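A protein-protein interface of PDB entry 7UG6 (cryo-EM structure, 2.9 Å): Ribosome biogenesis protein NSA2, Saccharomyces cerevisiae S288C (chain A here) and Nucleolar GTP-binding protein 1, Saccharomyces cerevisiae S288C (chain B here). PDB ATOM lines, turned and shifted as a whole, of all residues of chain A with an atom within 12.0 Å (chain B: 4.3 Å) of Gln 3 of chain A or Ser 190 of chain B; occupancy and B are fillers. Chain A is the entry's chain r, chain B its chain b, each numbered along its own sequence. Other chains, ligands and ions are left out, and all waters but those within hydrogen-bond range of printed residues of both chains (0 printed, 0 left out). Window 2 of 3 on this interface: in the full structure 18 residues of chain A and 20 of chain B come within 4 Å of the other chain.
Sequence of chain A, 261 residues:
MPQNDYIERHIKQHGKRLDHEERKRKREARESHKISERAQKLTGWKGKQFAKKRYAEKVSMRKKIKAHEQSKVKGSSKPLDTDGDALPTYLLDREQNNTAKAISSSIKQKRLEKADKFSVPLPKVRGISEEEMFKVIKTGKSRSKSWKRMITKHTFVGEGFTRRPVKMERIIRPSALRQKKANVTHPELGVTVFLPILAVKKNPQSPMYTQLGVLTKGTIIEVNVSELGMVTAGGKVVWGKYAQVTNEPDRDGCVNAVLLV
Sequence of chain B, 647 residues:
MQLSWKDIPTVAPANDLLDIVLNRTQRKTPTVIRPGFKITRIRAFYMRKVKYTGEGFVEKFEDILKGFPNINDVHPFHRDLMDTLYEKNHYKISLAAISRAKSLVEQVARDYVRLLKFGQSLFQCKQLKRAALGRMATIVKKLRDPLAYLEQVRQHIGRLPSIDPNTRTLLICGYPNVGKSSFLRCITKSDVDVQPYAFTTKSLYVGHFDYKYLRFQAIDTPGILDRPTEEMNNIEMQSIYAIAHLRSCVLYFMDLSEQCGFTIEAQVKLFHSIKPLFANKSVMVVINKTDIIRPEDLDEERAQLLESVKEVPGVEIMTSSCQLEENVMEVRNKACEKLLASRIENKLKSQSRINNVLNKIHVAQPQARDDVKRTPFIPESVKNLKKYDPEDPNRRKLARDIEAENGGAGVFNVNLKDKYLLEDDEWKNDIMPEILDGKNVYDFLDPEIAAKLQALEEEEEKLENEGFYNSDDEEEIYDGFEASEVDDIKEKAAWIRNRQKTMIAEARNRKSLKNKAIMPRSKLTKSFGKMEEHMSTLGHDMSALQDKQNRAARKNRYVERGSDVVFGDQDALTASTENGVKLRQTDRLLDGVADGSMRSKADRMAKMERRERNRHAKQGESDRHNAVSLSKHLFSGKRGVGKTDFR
Gln 3 of chain A touches just these residues of chain B: Arg 159, Leu 160, Pro 161, Ser 190, Tyr 205 and Val 206.
Printed residues of chain B within 4 Å of Asn 4 of chain A: Pro 161 (3.9 Å) and Tyr 205 (3.4 Å).
Of the printed residues of chain B, Asp 5 of chain A touches Arg 159.
Of the printed residues of chain B, Tyr 6 of chain A touches Arg 159.
Printed residues of chain B within 4 Å of Arg 9 of chain A: Asp 191 (3.9 Å) and Tyr 205 (3.9 Å).
Of chain A, only Pro 2, Gln 3, Asp 5 and Tyr 6 come within 4 Å of Arg 159 of chain B.
Of chain A, only Gln 3 (3.8 Å) comes within 4 Å of Leu 160 of chain B.
No residue of chain A comes within 4 Å of Lys 189 of chain B.
Of the printed residues of chain A, Asp 191 of chain B touches Arg 9.
Of chain A, only Gln 3 (3.6 Å), Asn 4 (3.4 Å) and Arg 9 (3.9 Å) come within 4 Å of Tyr 205 of chain B.
Of the printed residues of chain A, Val 206 of chain B touches Gln 3.
The nearest residue of chain A that does not touch Ser 190 of chain B is Arg 9 of chain A (6.0 Å).
The nearest printed residue of chain B that does not touch Asn 4 of chain A is Leu 160 of chain B (4.1 Å).
Among the printed residues, merely in contact across the chains: Asn 4 of chain A with Tyr 205 of chain B, Gln 3 of chain A with Tyr 205 of chain B, Tyr 6 of chain A with Arg 159 of chain B, Gln 3 of chain A with Leu 160 of chain B, Pro 2 of chain A with Arg 159 of chain B, Gln 3 of chain A with Pro 161 of chain B, Arg 9 of chain A with Tyr 205 of chain B, Arg 9 of chain A with Asp 191 of chain B and Asn 4 of chain A with Pro 161 of chain B.
The guanidinium group (NH2) of Arg 159 of chain B lies within salt-bridge range of the side-chain carboxylate (OD1) of Asp 5 of chain A, 2.8 Å away.
The side-chain amide nitrogen (NE2) of Gln 3 of chain A is in hydrogen-bond range of the side-chain hydroxyl (OG) of Ser 190 of chain B (3.4 Å).
O of Gln 3 of chain A lies close to O of Arg 159 of chain B, at 2.5 Å.
The backbone NH (N) of Val 206 of chain B lies within hydrogen-bond range of the side-chain amide oxygen (OE1) of Gln 3 of chain A, at 2.8 Å.
The backbone carbonyl oxygen (O) of Asn 4 of chain A sits at hydrogen-bond distance from the guanidinium group (NH1) of Arg 9 of chain A (2.5 Å).
The side-chain hydroxyl (OG) of Ser 190 of chain B sits at hydrogen-bond distance from the backbone carbonyl oxygen (O) of Val 206 of chain B (3.4 Å).
Of the 13 printed residues of chain B, 7 touch a printed residue of chain A.
Printed residues of chain A that touch a printed residue of chain B: Pro 2, Gln 3, Asn 4, Asp 5, Tyr 6 and Arg 9.
Hydrophobic or aromatic side chains of chain A within 4 Å of the printed part of chain B: Tyr 6.
Along chain A the printed residues that touch a printed residue of chain B span positions 2 to 9.
Among the printed residues, Asp or Glu carboxylates within 4 Å of a Lys or Arg side-chain nitrogen of the other chain: Asp 5 of chain A with Arg 159 of chain B (2.8 Å).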
ATOM      1  N   PRO A   2     -29.396  -0.764 -16.799  1.00  0.00           N
ATOM      2  CA  PRO A   2     -29.661  -2.183 -16.988  1.00  0.00           C
ATOM      3  C   PRO A   2     -30.274  -2.403 -18.363  1.00  0.00           C
ATOM      4  O   PRO A   2     -30.918  -1.485 -18.842  1.00  0.00           O
ATOM      5  CB  PRO A   2     -30.615  -2.477 -15.860  1.00  0.00           C
ATOM      6  CG  PRO A   2     -31.345  -1.243 -15.694  1.00  0.00           C
ATOM      7  CD  PRO A   2     -30.488  -0.113 -16.072  1.00  0.00           C
ATOM      8  N   GLN A   3     -30.063  -3.536 -19.024  1.00  0.00           N
ATOM      9  CA  GLN A   3     -30.367  -3.549 -20.444  1.00  0.00           C
ATOM     10  C   GLN A   3     -31.157  -4.740 -20.961  1.00  0.00           C
ATOM     11  O   GLN A   3     -31.862  -4.585 -21.952  1.00  0.00           O
ATOM     12  CB  GLN A   3     -29.079  -3.440 -21.258  1.00  0.00           C
ATOM     13  CG  GLN A   3     -28.013  -4.377 -20.829  1.00  0.00           C
ATOM     14  CD  GLN A   3     -26.660  -3.882 -21.202  1.00  0.00           C
ATOM     15  OE1 GLN A   3     -26.453  -3.404 -22.307  1.00  0.00           O
ATOM     16  NE2 GLN A   3     -25.722  -3.979 -20.279  1.00  0.00           N
ATOM     17  N   ASN A   4     -31.056  -5.923 -20.386  1.00  0.00           N
ATOM     18  CA  ASN A   4     -31.704  -7.050 -21.049  1.00  0.00           C
ATOM     19  C   ASN A   4     -32.083  -8.091 -20.017  1.00  0.00           C
ATOM     20  O   ASN A   4     -31.211  -8.841 -19.569  1.00  0.00           O
ATOM     21  CB  ASN A   4     -30.788  -7.668 -22.097  1.00  0.00           C
ATOM     22  CG  ASN A   4     -30.773  -6.903 -23.380  1.00  0.00           C
ATOM     23  OD1 ASN A   4     -31.813  -6.606 -23.951  1.00  0.00           O
ATOM     24  ND2 ASN A   4     -29.589  -6.601 -23.863  1.00  0.00           N
ATOM     25  N   ASP A   5     -33.370  -8.169 -19.683  1.00  0.00           N
ATOM     26  CA  ASP A   5     -33.851  -9.154 -18.719  1.00  0.00           C
ATOM     27  C   ASP A   5     -33.044  -9.069 -17.436  1.00  0.00           C
ATOM     28  O   ASP A   5     -32.623 -10.078 -16.878  1.00  0.00           O
ATOM     29  CB  ASP A   5     -33.790 -10.568 -19.295  1.00  0.00           C
ATOM     30  CG  ASP A   5     -34.790 -10.794 -20.407  1.00  0.00           C
ATOM     31  OD1 ASP A   5     -35.857 -10.145 -20.394  1.00  0.00           O
ATOM     32  OD2 ASP A   5     -34.513 -11.627 -21.297  1.00  0.00           O
ATOM     33  N   TYR A   6     -32.776  -7.844 -16.995  1.00  0.00           N
ATOM     34  CA  TYR A   6     -31.857  -7.658 -15.888  1.00  0.00           C
ATOM     35  C   TYR A   6     -32.438  -8.116 -14.567  1.00  0.00           C
ATOM     36  O   TYR A   6     -31.695  -8.246 -13.594  1.00  0.00           O
ATOM     37  CB  TYR A   6     -31.416  -6.202 -15.803  1.00  0.00           C
ATOM     38  CG  TYR A   6     -32.496  -5.174 -15.982  1.00  0.00           C
ATOM     39  CD1 TYR A   6     -32.832  -4.708 -17.235  1.00  0.00           C
ATOM     40  CD2 TYR A   6     -33.130  -4.614 -14.893  1.00  0.00           C
ATOM     41  CE1 TYR A   6     -33.794  -3.757 -17.399  1.00  0.00           C
ATOM     42  CE2 TYR A   6     -34.095  -3.666 -15.052  1.00  0.00           C
ATOM     43  CZ  TYR A   6     -34.422  -3.243 -16.301  1.00  0.00           C
ATOM     44  OH  TYR A   6     -35.385  -2.287 -16.456  1.00  0.00           O
ATOM     45  N   ILE A   7     -33.728  -8.427 -14.514  1.00  0.00           N
ATOM     46  CA  ILE A   7     -34.259  -8.972 -13.279  1.00  0.00           C
ATOM     47  C   ILE A   7     -34.114 -10.489 -13.241  1.00  0.00           C
ATOM     48  O   ILE A   7     -33.812 -11.038 -12.187  1.00  0.00           O
ATOM     49  CB  ILE A   7     -35.703  -8.512 -13.053  1.00  0.00           C
ATOM     50  CG1 ILE A   7     -35.717  -7.017 -12.772  1.00  0.00           C
ATOM     51  CG2 ILE A   7     -36.297  -9.208 -11.862  1.00  0.00           C
ATOM     52  CD1 ILE A   7     -34.945  -6.632 -11.558  1.00  0.00           C
ATOM     53  N   GLU A   8     -34.276 -11.208 -14.360  1.00  0.00           N
ATOM     54  CA  GLU A   8     -33.823 -12.600 -14.321  1.00  0.00           C
ATOM     55  C   GLU A   8     -32.339 -12.679 -14.029  1.00  0.00           C
ATOM     56  O   GLU A   8     -31.897 -13.565 -13.299  1.00  0.00           O
ATOM     57  CB  GLU A   8     -34.077 -13.396 -15.602  1.00  0.00           C
ATOM     58  CG  GLU A   8     -35.478 -13.784 -15.973  1.00  0.00           C
ATOM     59  CD  GLU A   8     -36.168 -12.731 -16.723  1.00  0.00           C
ATOM     60  OE1 GLU A   8     -35.511 -11.711 -16.996  1.00  0.00           O
ATOM     61  OE2 GLU A   8     -37.344 -12.937 -17.089  1.00  0.00           O
ATOM     62  N   ARG A   9     -31.548 -11.791 -14.614  1.00  0.00           N
ATOM     63  CA  ARG A   9     -30.130 -11.800 -14.308  1.00  0.00           C
ATOM     64  C   ARG A   9     -29.902 -11.532 -12.834  1.00  0.00           C
ATOM     65  O   ARG A   9     -29.035 -12.151 -12.214  1.00  0.00           O
ATOM     66  CB  ARG A   9     -29.394 -10.783 -15.168  1.00  0.00           C
ATOM     67  CG  ARG A   9     -29.019 -11.311 -16.529  1.00  0.00           C
ATOM     68  CD  ARG A   9     -29.145 -10.234 -17.576  1.00  0.00           C
ATOM     69  NE  ARG A   9     -28.186  -9.163 -17.346  1.00  0.00           N
ATOM     70  CZ  ARG A   9     -28.375  -7.904 -17.709  1.00  0.00           C
ATOM     71  NH1 ARG A   9     -29.493  -7.556 -18.317  1.00  0.00           N
ATOM     72  NH2 ARG A   9     -27.452  -6.991 -17.458  1.00  0.00           N
ATOM     73  N   HIS A  10     -30.689 -10.640 -12.241  1.00  0.00           N
ATOM     74  CA  HIS A  10     -30.518 -10.384 -10.819  1.00  0.00           C
ATOM     75  C   HIS A  10     -30.932 -11.580  -9.971  1.00  0.00           C
ATOM     76  O   HIS A  10     -30.256 -11.910  -8.994  1.00  0.00           O
ATOM     77  CB  HIS A  10     -31.295  -9.152 -10.400  1.00  0.00           C
ATOM     78  CG  HIS A  10     -31.072  -8.783  -8.975  1.00  0.00           C
ATOM     79  ND1 HIS A  10     -29.910  -8.195  -8.539  1.00  0.00           N
ATOM     80  CD2 HIS A  10     -31.841  -8.958  -7.880  1.00  0.00           C
ATOM     81  CE1 HIS A  10     -29.982  -8.002  -7.236  1.00  0.00           C
ATOM     82  NE2 HIS A  10     -31.144  -8.456  -6.812  1.00  0.00           N
ATOM     83  N   GLN A  13     -28.127 -14.162 -10.355  1.00  0.00           N
ATOM     84  CA  GLN A  13     -26.858 -13.802  -9.753  1.00  0.00           C
ATOM     85  C   GLN A  13     -26.931 -13.609  -8.247  1.00  0.00           C
ATOM     86  O   GLN A  13     -25.909 -13.758  -7.574  1.00  0.00           O
ATOM     87  CB  GLN A  13     -26.323 -12.524 -10.396  1.00  0.00           C
ATOM     88  CG  GLN A  13     -25.874 -12.697 -11.820  1.00  0.00           C
ATOM     89  CD  GLN A  13     -24.590 -13.461 -11.923  1.00  0.00           C
ATOM     90  OE1 GLN A  13     -23.694 -13.291 -11.106  1.00  0.00           O
ATOM     91  NE2 GLN A  13     -24.488 -14.317 -12.926  1.00  0.00           N
ATOM     92  N   HIS A  14     -28.094 -13.274  -7.699  1.00  0.00           N
ATOM     93  CA  HIS A  14     -28.205 -12.952  -6.288  1.00  0.00           C
ATOM     94  C   HIS A  14     -29.368 -13.622  -5.585  1.00  0.00           C
ATOM     95  O   HIS A  14     -29.477 -13.489  -4.365  1.00  0.00           O
ATOM     96  CB  HIS A  14     -28.330 -11.437  -6.096  1.00  0.00           C
ATOM     97  CG  HIS A  14     -27.315 -10.650  -6.856  1.00  0.00           C
ATOM     98  ND1 HIS A  14     -26.056 -10.396  -6.367  1.00  0.00           N
ATOM     99  CD2 HIS A  14     -27.369 -10.070  -8.075  1.00  0.00           C
ATOM    100  CE1 HIS A  14     -25.377  -9.687  -7.250  1.00  0.00           C
ATOM    101  NE2 HIS A  14     -26.152  -9.478  -8.296  1.00  0.00           N
ATOM    102  N   ARG B 159     -36.610  -1.936 -21.892  1.00  0.00           N
ATOM    103  CA  ARG B 159     -35.407  -2.504 -21.328  1.00  0.00           C
ATOM    104  C   ARG B 159     -34.235  -2.448 -22.281  1.00  0.00           C
ATOM    105  O   ARG B 159     -33.105  -2.371 -21.811  1.00  0.00           O
ATOM    106  CB  ARG B 159     -35.655  -3.945 -20.888  1.00  0.00           C
ATOM    107  CG  ARG B 159     -36.682  -4.042 -19.785  1.00  0.00           C
ATOM    108  CD  ARG B 159     -36.720  -5.393 -19.174  1.00  0.00           C
ATOM    109  NE  ARG B 159     -36.683  -6.438 -20.177  1.00  0.00           N
ATOM    110  CZ  ARG B 159     -37.684  -7.274 -20.403  1.00  0.00           C
ATOM    111  NH1 ARG B 159     -38.796  -7.171 -19.699  1.00  0.00           N
ATOM    112  NH2 ARG B 159     -37.577  -8.209 -21.330  1.00  0.00           N
ATOM    113  N   LEU B 160     -34.488  -2.397 -23.586  1.00  0.00           N
ATOM    114  CA  LEU B 160     -33.447  -2.413 -24.605  1.00  0.00           C
ATOM    115  C   LEU B 160     -32.350  -1.391 -24.323  1.00  0.00           C
ATOM    116  O   LEU B 160     -32.611  -0.326 -23.762  1.00  0.00           O
ATOM    117  CB  LEU B 160     -34.043  -2.121 -25.973  1.00  0.00           C
ATOM    118  CG  LEU B 160     -34.913  -3.207 -26.574  1.00  0.00           C
ATOM    119  CD1 LEU B 160     -35.293  -2.804 -27.972  1.00  0.00           C
ATOM    120  CD2 LEU B 160     -34.171  -4.510 -26.563  1.00  0.00           C
ATOM    121  N   PRO B 161     -31.115  -1.686 -24.716  1.00  0.00           N
ATOM    122  CA  PRO B 161     -30.019  -0.753 -24.479  1.00  0.00           C
ATOM    123  C   PRO B 161     -30.215   0.551 -25.229  1.00  0.00           C
ATOM    124  O   PRO B 161     -31.156   0.741 -25.999  1.00  0.00           O
ATOM    125  CB  PRO B 161     -28.799  -1.506 -24.996  1.00  0.00           C
ATOM    126  CG  PRO B 161     -29.195  -2.899 -25.039  1.00  0.00           C
ATOM    127  CD  PRO B 161     -30.639  -2.933 -25.320  1.00  0.00           C
ATOM    128  N   LEU B 184     -16.220  -7.931 -23.011  1.00  0.00           N
ATOM    129  CA  LEU B 184     -17.032  -6.818 -22.553  1.00  0.00           C
ATOM    130  C   LEU B 184     -16.968  -6.657 -21.044  1.00  0.00           C
ATOM    131  O   LEU B 184     -17.085  -5.536 -20.549  1.00  0.00           O
ATOM    132  CB  LEU B 184     -18.476  -6.975 -23.017  1.00  0.00           C
ATOM    133  CG  LEU B 184     -19.240  -5.657 -22.947  1.00  0.00           C
ATOM    134  CD1 LEU B 184     -18.677  -4.727 -23.955  1.00  0.00           C
ATOM    135  CD2 LEU B 184     -20.692  -5.850 -23.219  1.00  0.00           C
ATOM    136  N   ARG B 185     -16.781  -7.738 -20.287  1.00  0.00           N
ATOM    137  CA  ARG B 185     -16.640  -7.504 -18.857  1.00  0.00           C
ATOM    138  C   ARG B 185     -15.282  -6.916 -18.545  1.00  0.00           C
ATOM    139  O   ARG B 185     -15.129  -6.228 -17.531  1.00  0.00           O
ATOM    140  CB  ARG B 185     -16.850  -8.781 -18.036  1.00  0.00           C
ATOM    141  CG  ARG B 185     -15.915  -9.951 -18.310  1.00  0.00           C
ATOM    142  CD  ARG B 185     -14.631  -9.914 -17.476  1.00  0.00           C
ATOM    143  NE  ARG B 185     -13.806 -11.111 -17.632  1.00  0.00           N
ATOM    144  CZ  ARG B 185     -12.592 -11.247 -17.107  1.00  0.00           C
ATOM    145  NH1 ARG B 185     -12.071 -10.266 -16.387  1.00  0.00           N
ATOM    146  NH2 ARG B 185     -11.896 -12.359 -17.296  1.00  0.00           N
ATOM    147  N   THR B 188     -14.845  -2.855 -20.193  1.00  0.00           N
ATOM    148  CA  THR B 188     -15.776  -1.857 -19.699  1.00  0.00           C
ATOM    149  C   THR B 188     -16.574  -2.444 -18.549  1.00  0.00           C
ATOM    150  O   THR B 188     -16.552  -3.650 -18.302  1.00  0.00           O
ATOM    151  CB  THR B 188     -16.718  -1.361 -20.795  1.00  0.00           C
ATOM    152  OG1 THR B 188     -17.668  -0.453 -20.223  1.00  0.00           O
ATOM    153  CG2 THR B 188     -17.450  -2.499 -21.416  1.00  0.00           C
ATOM    154  N   LYS B 189     -17.254  -1.565 -17.827  1.00  0.00           N
ATOM    155  CA  LYS B 189     -18.145  -1.979 -16.753  1.00  0.00           C
ATOM    156  C   LYS B 189     -19.447  -2.458 -17.364  1.00  0.00           C
ATOM    157  O   LYS B 189     -20.236  -1.642 -17.844  1.00  0.00           O
ATOM    158  CB  LYS B 189     -18.404  -0.813 -15.806  1.00  0.00           C
ATOM    159  CG  LYS B 189     -17.188  -0.310 -15.067  1.00  0.00           C
ATOM    160  CD  LYS B 189     -17.401   1.114 -14.608  1.00  0.00           C
ATOM    161  CE  LYS B 189     -18.530   1.199 -13.610  1.00  0.00           C
ATOM    162  NZ  LYS B 189     -19.062   2.582 -13.493  1.00  0.00           N
ATOM    163  N   SER B 190     -19.673  -3.770 -17.364  1.00  0.00           N
ATOM    164  CA  SER B 190     -20.923  -4.347 -17.840  1.00  0.00           C
ATOM    165  C   SER B 190     -20.911  -5.829 -17.517  1.00  0.00           C
ATOM    166  O   SER B 190     -19.854  -6.463 -17.488  1.00  0.00           O
ATOM    167  CB  SER B 190     -21.120  -4.141 -19.341  1.00  0.00           C
ATOM    168  OG  SER B 190     -22.393  -4.598 -19.737  1.00  0.00           O
ATOM    169  N   ASP B 191     -22.102  -6.379 -17.293  1.00  0.00           N
ATOM    170  CA  ASP B 191     -22.266  -7.783 -16.932  1.00  0.00           C
ATOM    171  C   ASP B 191     -22.835  -8.520 -18.131  1.00  0.00           C
ATOM    172  O   ASP B 191     -23.941  -8.212 -18.584  1.00  0.00           O
ATOM    173  CB  ASP B 191     -23.184  -7.940 -15.718  1.00  0.00           C
ATOM    174  CG  ASP B 191     -23.534  -9.393 -15.435  1.00  0.00           C
ATOM    175  OD1 ASP B 191     -22.611 -10.233 -15.417  1.00  0.00           O
ATOM    176  OD2 ASP B 191     -24.734  -9.695 -15.242  1.00  0.00           O
ATOM    177  N   VAL B 192     -22.080  -9.482 -18.650  1.00  0.00           N
ATOM    178  CA  VAL B 192     -22.534 -10.340 -19.734  1.00  0.00           C
ATOM    179  C   VAL B 192     -22.340 -11.782 -19.303  1.00  0.00           C
ATOM    180  O   VAL B 192     -21.247 -12.164 -18.876  1.00  0.00           O
ATOM    181  CB  VAL B 192     -21.779 -10.064 -21.045  1.00  0.00           C
ATOM    182  CG1 VAL B 192     -22.291 -10.965 -22.152  1.00  0.00           C
ATOM    183  CG2 VAL B 192     -21.945  -8.629 -21.441  1.00  0.00           C
ATOM    184  N   TYR B 205     -25.626  -6.343 -25.942  1.00  0.00           N
ATOM    185  CA  TYR B 205     -25.214  -5.778 -24.671  1.00  0.00           C
ATOM    186  C   TYR B 205     -24.221  -4.664 -24.928  1.00  0.00           C
ATOM    187  O   TYR B 205     -23.330  -4.798 -25.764  1.00  0.00           O
ATOM    188  CB  TYR B 205     -24.605  -6.831 -23.767  1.00  0.00           C
ATOM    189  CG  TYR B 205     -25.646  -7.720 -23.152  1.00  0.00           C
ATOM    190  CD1 TYR B 205     -26.204  -8.758 -23.870  1.00  0.00           C
ATOM    191  CD2 TYR B 205     -26.092  -7.507 -21.861  1.00  0.00           C
ATOM    192  CE1 TYR B 205     -27.154  -9.560 -23.321  1.00  0.00           C
ATOM    193  CE2 TYR B 205     -27.043  -8.306 -21.309  1.00  0.00           C
ATOM    194  CZ  TYR B 205     -27.571  -9.330 -22.044  1.00  0.00           C
ATOM    195  OH  TYR B 205     -28.527 -10.139 -21.502  1.00  0.00           O
ATOM    196  N   VAL B 206     -24.385  -3.565 -24.216  1.00  0.00           N
ATOM    197  CA  VAL B 206     -23.585  -2.374 -24.429  1.00  0.00           C
ATOM    198  C   VAL B 206     -22.789  -2.086 -23.173  1.00  0.00           C
ATOM    199  O   VAL B 206     -23.287  -2.265 -22.059  1.00  0.00           O
ATOM    200  CB  VAL B 206     -24.468  -1.176 -24.799  1.00  0.00           C
ATOM    201  CG1 VAL B 206     -23.624  -0.018 -25.250  1.00  0.00           C
ATOM    202  CG2 VAL B 206     -25.376  -1.575 -25.887  1.00  0.00           C
ATOM    203  N   GLY B 207     -21.537  -1.679 -23.361  1.00  0.00           N
ATOM    204  CA  GLY B 207     -20.744  -1.120 -22.295  1.00  0.00           C
ATOM    205  C   GLY B 207     -20.127   0.178 -22.779  1.00  0.00           C
ATOM    206  O   GLY B 207     -20.251   0.540 -23.944  1.00  0.00           O
